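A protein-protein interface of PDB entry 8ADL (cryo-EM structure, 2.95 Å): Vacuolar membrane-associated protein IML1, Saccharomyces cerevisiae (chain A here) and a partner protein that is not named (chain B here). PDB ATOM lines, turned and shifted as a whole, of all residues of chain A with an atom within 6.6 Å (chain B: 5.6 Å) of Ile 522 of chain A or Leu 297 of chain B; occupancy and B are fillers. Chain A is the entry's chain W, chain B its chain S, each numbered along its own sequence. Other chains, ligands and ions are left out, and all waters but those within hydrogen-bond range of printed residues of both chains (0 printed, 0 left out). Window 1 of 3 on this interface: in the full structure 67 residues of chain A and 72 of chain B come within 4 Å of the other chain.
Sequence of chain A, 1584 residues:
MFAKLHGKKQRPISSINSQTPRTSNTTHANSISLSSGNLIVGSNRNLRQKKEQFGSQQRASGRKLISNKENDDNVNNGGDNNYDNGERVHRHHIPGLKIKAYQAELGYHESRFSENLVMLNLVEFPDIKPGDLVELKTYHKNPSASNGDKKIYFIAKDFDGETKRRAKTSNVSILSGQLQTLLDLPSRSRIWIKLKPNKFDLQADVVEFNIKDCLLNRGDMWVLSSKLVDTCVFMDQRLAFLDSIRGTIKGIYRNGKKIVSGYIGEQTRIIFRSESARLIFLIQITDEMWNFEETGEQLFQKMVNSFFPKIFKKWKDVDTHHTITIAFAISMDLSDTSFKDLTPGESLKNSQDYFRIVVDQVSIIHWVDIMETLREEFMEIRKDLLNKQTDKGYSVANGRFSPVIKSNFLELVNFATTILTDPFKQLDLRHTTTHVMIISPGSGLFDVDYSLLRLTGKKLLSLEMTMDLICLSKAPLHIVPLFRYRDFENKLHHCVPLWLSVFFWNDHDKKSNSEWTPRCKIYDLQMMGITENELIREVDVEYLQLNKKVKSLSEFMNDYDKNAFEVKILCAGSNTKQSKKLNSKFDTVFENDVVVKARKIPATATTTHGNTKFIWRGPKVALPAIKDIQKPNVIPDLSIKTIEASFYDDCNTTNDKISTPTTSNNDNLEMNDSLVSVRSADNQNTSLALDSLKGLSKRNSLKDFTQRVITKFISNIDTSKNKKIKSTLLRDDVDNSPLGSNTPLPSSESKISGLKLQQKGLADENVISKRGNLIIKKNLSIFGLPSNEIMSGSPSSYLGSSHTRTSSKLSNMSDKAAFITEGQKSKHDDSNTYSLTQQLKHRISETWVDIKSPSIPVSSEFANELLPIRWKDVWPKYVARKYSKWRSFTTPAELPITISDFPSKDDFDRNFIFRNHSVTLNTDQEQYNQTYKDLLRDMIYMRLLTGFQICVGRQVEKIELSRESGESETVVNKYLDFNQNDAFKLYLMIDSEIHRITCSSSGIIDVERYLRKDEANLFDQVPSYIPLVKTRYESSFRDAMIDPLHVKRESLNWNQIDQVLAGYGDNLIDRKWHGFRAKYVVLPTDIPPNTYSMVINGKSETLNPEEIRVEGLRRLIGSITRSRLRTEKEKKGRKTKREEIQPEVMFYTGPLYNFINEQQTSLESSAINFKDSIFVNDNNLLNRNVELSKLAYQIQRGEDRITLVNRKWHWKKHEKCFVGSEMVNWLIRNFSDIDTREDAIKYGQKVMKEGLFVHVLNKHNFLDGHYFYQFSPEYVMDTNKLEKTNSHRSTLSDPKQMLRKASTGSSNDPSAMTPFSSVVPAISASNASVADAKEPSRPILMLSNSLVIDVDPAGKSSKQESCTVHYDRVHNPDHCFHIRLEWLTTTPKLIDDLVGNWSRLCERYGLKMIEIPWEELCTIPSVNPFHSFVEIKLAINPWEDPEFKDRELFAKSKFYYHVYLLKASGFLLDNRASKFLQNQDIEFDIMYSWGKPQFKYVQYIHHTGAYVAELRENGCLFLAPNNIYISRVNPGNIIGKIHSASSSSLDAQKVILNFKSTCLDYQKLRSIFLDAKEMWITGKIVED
Of the printed residues of chain B, Cys 520 of chain A touches Met 263 (3.7 Å), His 296 (3.5 Å) and Tyr 300 (3.7 Å).
Ile 522 of chain A touches just these residues of chain B: Trp 259 (3.5 Å), Met 263 (3.7 Å), Leu 297 (3.7 Å) and Tyr 300 (3.6 Å).
Of the printed residues of chain B, Gln 526 of chain A touches Tyr 300.
Leu 251 of chain B touches none of the printed residues of chain A.
Printed residues of chain A within 4 Å of Asn 258 of chain B: Lys 521.
Of the printed residues of chain A, Met 263 of chain B touches Cys 520 (3.7 Å) and Ile 522 (3.7 Å).
Arg 295 of chain B touches none of the printed residues of chain A.
Leu 297 of chain B touches just one residue of chain A: Ile 522.
Tyr 300 of chain B touches Glu 294 of chain A (OH to OE2, 3.6 Å).
CB of Cys 520 of chain A touches CE of Met 263 of chain B (3.7 Å).
N of Cys 520 of chain A touches CD2 of His 296 of chain B, at 3.5 Å.
O of Cys 520 of chain A touches OH of Tyr 300 of chain B (3.7 Å).
Trp 259 of chain B touches Ile 522 of chain A (NE1 to CG2, 3.5 Å).
Ile 522 of chain A touches Met 263 of chain B (CD1 to SD, 3.7 Å).
Ile 522 of chain A touches Tyr 300 of chain B (CD1 to CD2, 3.6 Å).
Ile 254 of chain B touches Asp 524 of chain A.
Cys 302 of chain B touches Leu 525 of chain A (SG to CD1, 3.7 Å).
Tyr 300 of chain B touches Gln 526 of chain A (CE1 to CB, 3.97 Å).
O of Lys 521 of chain A lies close to O of Asn 258 of chain B (3.2 Å).
The backbone NH of Met 263 of chain B is in hydrogen-bond range of the side-chain sulfur of Cys 293 of chain B, 3.7 Å away.
The backbone carbonyl oxygen (O) of Glu 292 of chain B lies within hydrogen-bond range of a ring nitrogen (ND1) of His 296 of chain B (2.4 Å).
O of Leu 297 of chain B sits at hydrogen-bond distance from N of Cys 302 of chain B.
The side-chain sulfur (SG) of Cys 302 of chain B is in hydrogen-bond range of the backbone carbonyl oxygen (O) of Tyr 300 of chain B, at 3.6 Å.
Printed residues of chain B that touch a printed residue of chain A: Ile 254, Asn 258, Trp 259, Met 263, His 296, Leu 297, Tyr 300 and Cys 302.
Hydrophobic or aromatic side chains of chain B within 4 Å of the printed part of chain A: Ile 254, Trp 259, Met 263, His 296, Leu 297 and Tyr 300.
Of the 9 printed residues of chain A, 7 touch a printed residue of chain B.
Hydrophobic or aromatic side chains of chain A within 4 Å of the printed part of chain B: Ile 522 and Leu 525.
Among the printed residues, no Asp or Glu carboxylate lies within 4 Å of a Lys or Arg side-chain nitrogen of the other chain.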
ATOM      1  N   GLU A 294      14.929 -20.364 -16.607  1.00  0.00           N
ATOM      2  CA  GLU A 294      14.112 -19.154 -16.538  1.00  0.00           C
ATOM      3  C   GLU A 294      12.726 -19.429 -15.963  1.00  0.00           C
ATOM      4  O   GLU A 294      12.114 -18.532 -15.371  1.00  0.00           O
ATOM      5  CB  GLU A 294      13.990 -18.520 -17.925  1.00  0.00           C
ATOM      6  CG  GLU A 294      15.281 -17.915 -18.448  1.00  0.00           C
ATOM      7  CD  GLU A 294      16.001 -18.826 -19.419  1.00  0.00           C
ATOM      8  OE1 GLU A 294      15.613 -20.007 -19.526  1.00  0.00           O
ATOM      9  OE2 GLU A 294      16.955 -18.360 -20.077  1.00  0.00           O
ATOM     10  N   CYS A 520      18.261 -17.314 -24.796  1.00  0.00           N
ATOM     11  CA  CYS A 520      19.616 -16.879 -24.488  1.00  0.00           C
ATOM     12  C   CYS A 520      19.784 -16.788 -22.980  1.00  0.00           C
ATOM     13  O   CYS A 520      18.930 -16.220 -22.290  1.00  0.00           O
ATOM     14  CB  CYS A 520      19.927 -15.527 -25.136  1.00  0.00           C
ATOM     15  SG  CYS A 520      20.322 -15.608 -26.895  1.00  0.00           S
ATOM     16  N   LYS A 521      20.878 -17.345 -22.473  1.00  0.00           N
ATOM     17  CA  LYS A 521      21.096 -17.472 -21.039  1.00  0.00           C
ATOM     18  C   LYS A 521      21.971 -16.320 -20.566  1.00  0.00           C
ATOM     19  O   LYS A 521      23.122 -16.191 -20.996  1.00  0.00           O
ATOM     20  CB  LYS A 521      21.737 -18.815 -20.694  1.00  0.00           C
ATOM     21  CG  LYS A 521      20.744 -19.867 -20.227  1.00  0.00           C
ATOM     22  CD  LYS A 521      21.427 -21.194 -19.942  1.00  0.00           C
ATOM     23  CE  LYS A 521      20.509 -22.131 -19.173  1.00  0.00           C
ATOM     24  NZ  LYS A 521      20.094 -21.562 -17.863  1.00  0.00           N
ATOM     25  N   ILE A 522      21.422 -15.486 -19.692  1.00  0.00           N
ATOM     26  CA  ILE A 522      22.184 -14.474 -18.972  1.00  0.00           C
ATOM     27  C   ILE A 522      22.016 -14.785 -17.493  1.00  0.00           C
ATOM     28  O   ILE A 522      20.978 -14.471 -16.896  1.00  0.00           O
ATOM     29  CB  ILE A 522      21.731 -13.047 -19.297  1.00  0.00           C
ATOM     30  CG1 ILE A 522      21.804 -12.787 -20.801  1.00  0.00           C
ATOM     31  CG2 ILE A 522      22.591 -12.051 -18.549  1.00  0.00           C
ATOM     32  CD1 ILE A 522      21.368 -11.396 -21.193  1.00  0.00           C
ATOM     33  N   TYR A 523      23.028 -15.416 -16.898  1.00  0.00           N
ATOM     34  CA  TYR A 523      22.886 -15.924 -15.539  1.00  0.00           C
ATOM     35  C   TYR A 523      22.955 -14.806 -14.505  1.00  0.00           C
ATOM     36  O   TYR A 523      22.245 -14.851 -13.495  1.00  0.00           O
ATOM     37  CB  TYR A 523      23.952 -16.983 -15.259  1.00  0.00           C
ATOM     38  CG  TYR A 523      23.591 -17.903 -14.119  1.00  0.00           C
ATOM     39  CD1 TYR A 523      22.569 -18.835 -14.251  1.00  0.00           C
ATOM     40  CD2 TYR A 523      24.281 -17.850 -12.913  1.00  0.00           C
ATOM     41  CE1 TYR A 523      22.233 -19.677 -13.211  1.00  0.00           C
ATOM     42  CE2 TYR A 523      23.955 -18.694 -11.866  1.00  0.00           C
ATOM     43  CZ  TYR A 523      22.932 -19.607 -12.022  1.00  0.00           C
ATOM     44  OH  TYR A 523      22.602 -20.448 -10.985  1.00  0.00           O
ATOM     45  N   ASP A 524      23.796 -13.797 -14.737  1.00  0.00           N
ATOM     46  CA  ASP A 524      23.980 -12.754 -13.736  1.00  0.00           C
ATOM     47  C   ASP A 524      22.803 -11.790 -13.677  1.00  0.00           C
ATOM     48  O   ASP A 524      22.649 -11.085 -12.674  1.00  0.00           O
ATOM     49  CB  ASP A 524      25.270 -11.984 -14.012  1.00  0.00           C
ATOM     50  CG  ASP A 524      26.509 -12.805 -13.728  1.00  0.00           C
ATOM     51  OD1 ASP A 524      26.370 -14.006 -13.416  1.00  0.00           O
ATOM     52  OD2 ASP A 524      27.623 -12.249 -13.819  1.00  0.00           O
ATOM     53  N   LEU A 525      21.973 -11.738 -14.719  1.00  0.00           N
ATOM     54  CA  LEU A 525      20.772 -10.911 -14.691  1.00  0.00           C
ATOM     55  C   LEU A 525      19.521 -11.691 -14.319  1.00  0.00           C
ATOM     56  O   LEU A 525      18.599 -11.114 -13.732  1.00  0.00           O
ATOM     57  CB  LEU A 525      20.558 -10.219 -16.042  1.00  0.00           C
ATOM     58  CG  LEU A 525      21.513  -9.057 -16.330  1.00  0.00           C
ATOM     59  CD1 LEU A 525      21.441  -8.621 -17.785  1.00  0.00           C
ATOM     60  CD2 LEU A 525      21.216  -7.891 -15.401  1.00  0.00           C
ATOM     61  N   GLN A 526      19.461 -12.981 -14.657  1.00  0.00           N
ATOM     62  CA  GLN A 526      18.356 -13.814 -14.193  1.00  0.00           C
ATOM     63  C   GLN A 526      18.441 -14.040 -12.688  1.00  0.00           C
ATOM     64  O   GLN A 526      17.436 -13.926 -11.977  1.00  0.00           O
ATOM     65  CB  GLN A 526      18.348 -15.143 -14.949  1.00  0.00           C
ATOM     66  CG  GLN A 526      17.556 -16.255 -14.277  1.00  0.00           C
ATOM     67  CD  GLN A 526      17.826 -17.614 -14.891  1.00  0.00           C
ATOM     68  OE1 GLN A 526      18.438 -17.718 -15.953  1.00  0.00           O
ATOM     69  NE2 GLN A 526      17.368 -18.667 -14.222  1.00  0.00           N
ATOM     70  N   MET A 527      19.636 -14.349 -12.185  1.00  0.00           N
ATOM     71  CA  MET A 527      19.838 -14.558 -10.758  1.00  0.00           C
ATOM     72  C   MET A 527      20.063 -13.262  -9.994  1.00  0.00           C
ATOM     73  O   MET A 527      20.153 -13.311  -8.761  1.00  0.00           O
ATOM     74  CB  MET A 527      21.020 -15.501 -10.518  1.00  0.00           C
ATOM     75  CG  MET A 527      20.868 -16.865 -11.164  1.00  0.00           C
ATOM     76  SD  MET A 527      19.605 -17.866 -10.358  1.00  0.00           S
ATOM     77  CE  MET A 527      20.560 -18.643  -9.057  1.00  0.00           C
ATOM     78  N   LEU B 251      28.068  -3.992 -19.876  1.00  0.00           N
ATOM     79  CA  LEU B 251      27.875  -5.362 -20.337  1.00  0.00           C
ATOM     80  C   LEU B 251      29.153  -6.191 -20.383  1.00  0.00           C
ATOM     81  O   LEU B 251      29.062  -7.412 -20.549  1.00  0.00           O
ATOM     82  CB  LEU B 251      27.226  -5.361 -21.725  1.00  0.00           C
ATOM     83  CG  LEU B 251      25.760  -4.929 -21.800  1.00  0.00           C
ATOM     84  CD1 LEU B 251      25.306  -4.803 -23.243  1.00  0.00           C
ATOM     85  CD2 LEU B 251      24.874  -5.908 -21.057  1.00  0.00           C
ATOM     86  N   ILE B 254      29.353  -8.368 -17.052  1.00  0.00           N
ATOM     87  CA  ILE B 254      28.309  -9.374 -16.885  1.00  0.00           C
ATOM     88  C   ILE B 254      28.629 -10.649 -17.659  1.00  0.00           C
ATOM     89  O   ILE B 254      28.044 -11.703 -17.378  1.00  0.00           O
ATOM     90  CB  ILE B 254      26.956  -8.786 -17.326  1.00  0.00           C
ATOM     91  CG1 ILE B 254      26.839  -7.337 -16.865  1.00  0.00           C
ATOM     92  CG2 ILE B 254      25.786  -9.562 -16.735  1.00  0.00           C
ATOM     93  CD1 ILE B 254      25.563  -6.668 -17.300  1.00  0.00           C
ATOM     94  N   ASN B 258      28.458 -18.648 -19.758  1.00  0.00           N
ATOM     95  CA  ASN B 258      27.148 -19.122 -20.187  1.00  0.00           C
ATOM     96  C   ASN B 258      26.451 -18.204 -21.185  1.00  0.00           C
ATOM     97  O   ASN B 258      25.323 -18.504 -21.588  1.00  0.00           O
ATOM     98  CB  ASN B 258      26.241 -19.331 -18.971  1.00  0.00           C
ATOM     99  CG  ASN B 258      26.648 -20.534 -18.147  1.00  0.00           C
ATOM    100  OD1 ASN B 258      27.075 -21.553 -18.691  1.00  0.00           O
ATOM    101  ND2 ASN B 258      26.518 -20.425 -16.830  1.00  0.00           N
ATOM    102  N   TRP B 259      27.072 -17.094 -21.580  1.00  0.00           N
ATOM    103  CA  TRP B 259      26.431 -16.186 -22.520  1.00  0.00           C
ATOM    104  C   TRP B 259      26.419 -16.783 -23.925  1.00  0.00           C
ATOM    105  O   TRP B 259      27.246 -17.631 -24.271  1.00  0.00           O
ATOM    106  CB  TRP B 259      27.137 -14.832 -22.520  1.00  0.00           C
ATOM    107  CG  TRP B 259      26.577 -13.904 -21.493  1.00  0.00           C
ATOM    108  CD1 TRP B 259      26.158 -14.233 -20.238  1.00  0.00           C
ATOM    109  CD2 TRP B 259      26.364 -12.496 -21.630  1.00  0.00           C
ATOM    110  NE1 TRP B 259      25.706 -13.117 -19.580  1.00  0.00           N
ATOM    111  CE2 TRP B 259      25.818 -12.037 -20.415  1.00  0.00           C
ATOM    112  CE3 TRP B 259      26.580 -11.580 -22.661  1.00  0.00           C
ATOM    113  CZ2 TRP B 259      25.488 -10.701 -20.203  1.00  0.00           C
ATOM    114  CZ3 TRP B 259      26.250 -10.255 -22.448  1.00  0.00           C
ATOM    115  CH2 TRP B 259      25.711  -9.827 -21.228  1.00  0.00           C
ATOM    116  N   MET B 263      25.497 -12.883 -28.697  1.00  0.00           N
ATOM    117  CA  MET B 263      25.391 -11.761 -27.770  1.00  0.00           C
ATOM    118  C   MET B 263      26.769 -11.283 -27.331  1.00  0.00           C
ATOM    119  O   MET B 263      27.000 -10.077 -27.193  1.00  0.00           O
ATOM    120  CB  MET B 263      24.552 -12.172 -26.564  1.00  0.00           C
ATOM    121  CG  MET B 263      23.816 -11.020 -25.914  1.00  0.00           C
ATOM    122  SD  MET B 263      22.709 -11.566 -24.605  1.00  0.00           S
ATOM    123  CE  MET B 263      21.300 -12.080 -25.576  1.00  0.00           C
ATOM    124  N   ILE B 266      27.942  -9.143 -29.944  1.00  0.00           N
ATOM    125  CA  ILE B 266      27.229  -7.866 -30.002  1.00  0.00           C
ATOM    126  C   ILE B 266      27.757  -6.903 -28.936  1.00  0.00           C
ATOM    127  O   ILE B 266      27.795  -5.684 -29.168  1.00  0.00           O
ATOM    128  CB  ILE B 266      25.700  -8.083 -29.893  1.00  0.00           C
ATOM    129  CG1 ILE B 266      25.198  -8.959 -31.034  1.00  0.00           C
ATOM    130  CG2 ILE B 266      24.923  -6.770 -29.950  1.00  0.00           C
ATOM    131  CD1 ILE B 266      25.558  -8.451 -32.397  1.00  0.00           C
ATOM    132  N   ILE B 270      27.839  -2.147 -28.712  1.00  0.00           N
ATOM    133  CA  ILE B 270      26.692  -1.367 -28.215  1.00  0.00           C
ATOM    134  C   ILE B 270      27.271  -0.143 -27.516  1.00  0.00           C
ATOM    135  O   ILE B 270      27.465  -0.101 -26.297  1.00  0.00           O
ATOM    136  CB  ILE B 270      25.780  -2.191 -27.301  1.00  0.00           C
ATOM    137  CG1 ILE B 270      25.393  -3.509 -27.972  1.00  0.00           C
ATOM    138  CG2 ILE B 270      24.525  -1.396 -26.943  1.00  0.00           C
ATOM    139  CD1 ILE B 270      24.473  -4.369 -27.131  1.00  0.00           C
ATOM    140  N   GLU B 292      17.222 -10.806 -32.317  1.00  0.00           N
ATOM    141  CA  GLU B 292      16.812 -11.693 -31.229  1.00  0.00           C
ATOM    142  C   GLU B 292      17.649 -11.475 -29.971  1.00  0.00           C
ATOM    143  O   GLU B 292      17.128 -11.567 -28.854  1.00  0.00           O
ATOM    144  CB  GLU B 292      16.890 -13.149 -31.687  1.00  0.00           C
ATOM    145  CG  GLU B 292      15.744 -13.575 -32.590  1.00  0.00           C
ATOM    146  CD  GLU B 292      14.635 -14.278 -31.832  1.00  0.00           C
ATOM    147  OE1 GLU B 292      14.647 -14.234 -30.583  1.00  0.00           O
ATOM    148  OE2 GLU B 292      13.751 -14.873 -32.483  1.00  0.00           O
ATOM    149  N   CYS B 293      18.941 -11.167 -30.125  1.00  0.00           N
ATOM    150  CA  CYS B 293      19.780 -10.897 -28.958  1.00  0.00           C
ATOM    151  C   CYS B 293      19.406  -9.576 -28.294  1.00  0.00           C
ATOM    152  O   CYS B 293      19.405  -9.474 -27.060  1.00  0.00           O
ATOM    153  CB  CYS B 293      21.257 -10.901 -29.351  1.00  0.00           C
ATOM    154  SG  CYS B 293      21.934 -12.542 -29.699  1.00  0.00           S
ATOM    155  N   ILE B 294      19.082  -8.556 -29.095  1.00  0.00           N
ATOM    156  CA  ILE B 294      18.599  -7.294 -28.539  1.00  0.00           C
ATOM    157  C   ILE B 294      17.257  -7.496 -27.842  1.00  0.00           C
ATOM    158  O   ILE B 294      17.001  -6.913 -26.782  1.00  0.00           O
ATOM    159  CB  ILE B 294      18.533  -6.224 -29.649  1.00  0.00           C
ATOM    160  CG1 ILE B 294      19.945  -5.827 -30.087  1.00  0.00           C
ATOM    161  CG2 ILE B 294      17.770  -4.982 -29.203  1.00  0.00           C
ATOM    162  CD1 ILE B 294      20.789  -5.237 -28.977  1.00  0.00           C
ATOM    163  N   ARG B 295      16.405  -8.367 -28.391  1.00  0.00           N
ATOM    164  CA  ARG B 295      15.142  -8.693 -27.732  1.00  0.00           C
ATOM    165  C   ARG B 295      15.369  -9.411 -26.405  1.00  0.00           C
ATOM    166  O   ARG B 295      14.677  -9.135 -25.419  1.00  0.00           O
ATOM    167  CB  ARG B 295      14.274  -9.540 -28.657  1.00  0.00           C
ATOM    168  CG  ARG B 295      13.404  -8.729 -29.595  1.00  0.00           C
ATOM    169  CD  ARG B 295      12.557  -9.638 -30.460  1.00  0.00           C
ATOM    170  NE  ARG B 295      11.251  -9.865 -29.854  1.00  0.00           N
ATOM    171  CZ  ARG B 295      10.585 -11.010 -29.910  1.00  0.00           C
ATOM    172  NH1 ARG B 295      11.074 -12.063 -30.544  1.00  0.00           N
ATOM    173  NH2 ARG B 295       9.398 -11.101 -29.315  1.00  0.00           N
ATOM    174  N   HIS B 296      16.331 -10.336 -26.364  1.00  0.00           N
ATOM    175  CA  HIS B 296      16.645 -11.032 -25.118  1.00  0.00           C
ATOM    176  C   HIS B 296      17.213 -10.079 -24.074  1.00  0.00           C
ATOM    177  O   HIS B 296      16.918 -10.211 -22.880  1.00  0.00           O
ATOM    178  CB  HIS B 296      17.625 -12.173 -25.383  1.00  0.00           C
ATOM    179  CG  HIS B 296      17.011 -13.353 -26.068  1.00  0.00           C
ATOM    180  ND1 HIS B 296      17.045 -13.521 -27.436  1.00  0.00           N
ATOM    181  CD2 HIS B 296      16.359 -14.431 -25.572  1.00  0.00           C
ATOM    182  CE1 HIS B 296      16.433 -14.648 -27.754  1.00  0.00           C
ATOM    183  NE2 HIS B 296      16.007 -15.219 -26.642  1.00  0.00           N
ATOM    184  N   LEU B 297      18.027  -9.112 -24.503  1.00  0.00           N
ATOM    185  CA  LEU B 297      18.547  -8.122 -23.565  1.00  0.00           C
ATOM    186  C   LEU B 297      17.458  -7.155 -23.109  1.00  0.00           C
ATOM    187  O   LEU B 297      17.521  -6.635 -21.988  1.00  0.00           O
ATOM    188  CB  LEU B 297      19.705  -7.359 -24.205  1.00  0.00           C
ATOM    189  CG  LEU B 297      21.056  -8.074 -24.245  1.00  0.00           C
ATOM    190  CD1 LEU B 297      21.976  -7.424 -25.266  1.00  0.00           C
ATOM    191  CD2 LEU B 297      21.701  -8.074 -22.869  1.00  0.00           C
ATOM    192  N   ILE B 298      16.464  -6.901 -23.962  1.00  0.00           N
ATOM    193  CA  ILE B 298      15.285  -6.135 -23.564  1.00  0.00           C
ATOM    194  C   ILE B 298      14.480  -6.904 -22.522  1.00  0.00           C
ATOM    195  O   ILE B 298      13.965  -6.322 -21.558  1.00  0.00           O
ATOM    196  CB  ILE B 298      14.448  -5.781 -24.813  1.00  0.00           C
ATOM    197  CG1 ILE B 298      15.057  -4.584 -25.544  1.00  0.00           C
ATOM    198  CG2 ILE B 298      12.990  -5.487 -24.469  1.00  0.00           C
ATOM    199  CD1 ILE B 298      14.681  -4.507 -27.008  1.00  0.00           C
ATOM    200  N   TYR B 299      14.393  -8.230 -22.687  1.00  0.00           N
ATOM    201  CA  TYR B 299      13.642  -9.083 -21.768  1.00  0.00           C
ATOM    202  C   TYR B 299      14.209  -9.039 -20.351  1.00  0.00           C
ATOM    203  O   TYR B 299      13.469  -9.237 -19.380  1.00  0.00           O
ATOM    204  CB  TYR B 299      13.619 -10.517 -22.299  1.00  0.00           C
ATOM    205  CG  TYR B 299      12.974 -11.506 -21.361  1.00  0.00           C
ATOM    206  CD1 TYR B 299      11.601 -11.501 -21.160  1.00  0.00           C
ATOM    207  CD2 TYR B 299      13.736 -12.444 -20.675  1.00  0.00           C
ATOM    208  CE1 TYR B 299      11.001 -12.404 -20.304  1.00  0.00           C
ATOM    209  CE2 TYR B 299      13.145 -13.352 -19.812  1.00  0.00           C
ATOM    210  CZ  TYR B 299      11.777 -13.325 -19.630  1.00  0.00           C
ATOM    211  OH  TYR B 299      11.182 -14.225 -18.776  1.00  0.00           O
ATOM    212  N   TYR B 300      15.507  -8.777 -20.209  1.00  0.00           N
ATOM    213  CA  TYR B 300      16.136  -8.647 -18.903  1.00  0.00           C
ATOM    214  C   TYR B 300      16.213  -7.195 -18.439  1.00  0.00           C
ATOM    215  O   TYR B 300      16.883  -6.913 -17.440  1.00  0.00           O
ATOM    216  CB  TYR B 300      17.532  -9.268 -18.927  1.00  0.00           C
ATOM    217  CG  TYR B 300      17.528 -10.778 -18.985  1.00  0.00           C
ATOM    218  CD1 TYR B 300      17.063 -11.533 -17.915  1.00  0.00           C
ATOM    219  CD2 TYR B 300      17.975 -11.450 -20.117  1.00  0.00           C
ATOM    220  CE1 TYR B 300      17.056 -12.918 -17.967  1.00  0.00           C
ATOM    221  CE2 TYR B 300      17.972 -12.832 -20.178  1.00  0.00           C
ATOM    222  CZ  TYR B 300      17.510 -13.559 -19.101  1.00  0.00           C
ATOM    223  OH  TYR B 300      17.504 -14.933 -19.158  1.00  0.00           O
ATOM    224  N   LYS B 301      15.547  -6.279 -19.158  1.00  0.00           N
ATOM    225  CA  LYS B 301      15.393  -4.865 -18.783  1.00  0.00           C
ATOM    226  C   LYS B 301      16.736  -4.146 -18.640  1.00  0.00           C
ATOM    227  O   LYS B 301      17.042  -3.550 -17.605  1.00  0.00           O
ATOM    228  CB  LYS B 301      14.557  -4.722 -17.508  1.00  0.00           C
ATOM    229  CG  LYS B 301      13.168  -5.334 -17.606  1.00  0.00           C
ATOM    230  CD  LYS B 301      12.290  -4.566 -18.581  1.00  0.00           C
ATOM    231  CE  LYS B 301      11.977  -3.172 -18.064  1.00  0.00           C
ATOM    232  NZ  LYS B 301      11.135  -3.209 -16.837  1.00  0.00           N
ATOM    233  N   CYS B 302      17.547  -4.204 -19.698  1.00  0.00           N
ATOM    234  CA  CYS B 302      18.867  -3.581 -19.663  1.00  0.00           C
ATOM    235  C   CYS B 302      19.240  -2.804 -20.917  1.00  0.00           C
ATOM    236  O   CYS B 302      20.233  -2.072 -20.878  1.00  0.00           O
ATOM    237  CB  CYS B 302      19.947  -4.639 -19.398  1.00  0.00           C
ATOM    238  SG  CYS B 302      19.998  -5.223 -17.691  1.00  0.00           S
ATOM    239  N   VAL B 303      18.498  -2.924 -22.016  1.00  0.00           N
ATOM    240  CA  VAL B 303      18.783  -2.206 -23.254  1.00  0.00           C
ATOM    241  C   VAL B 303      17.514  -1.507 -23.721  1.00  0.00           C
ATOM    242  O   VAL B 303      16.458  -2.139 -23.832  1.00  0.00           O
ATOM    243  CB  VAL B 303      19.315  -3.150 -24.354  1.00  0.00           C
ATOM    244  CG1 VAL B 303      19.481  -2.406 -25.666  1.00  0.00           C
ATOM    245  CG2 VAL B 303      20.644  -3.768 -23.941  1.00  0.00           C
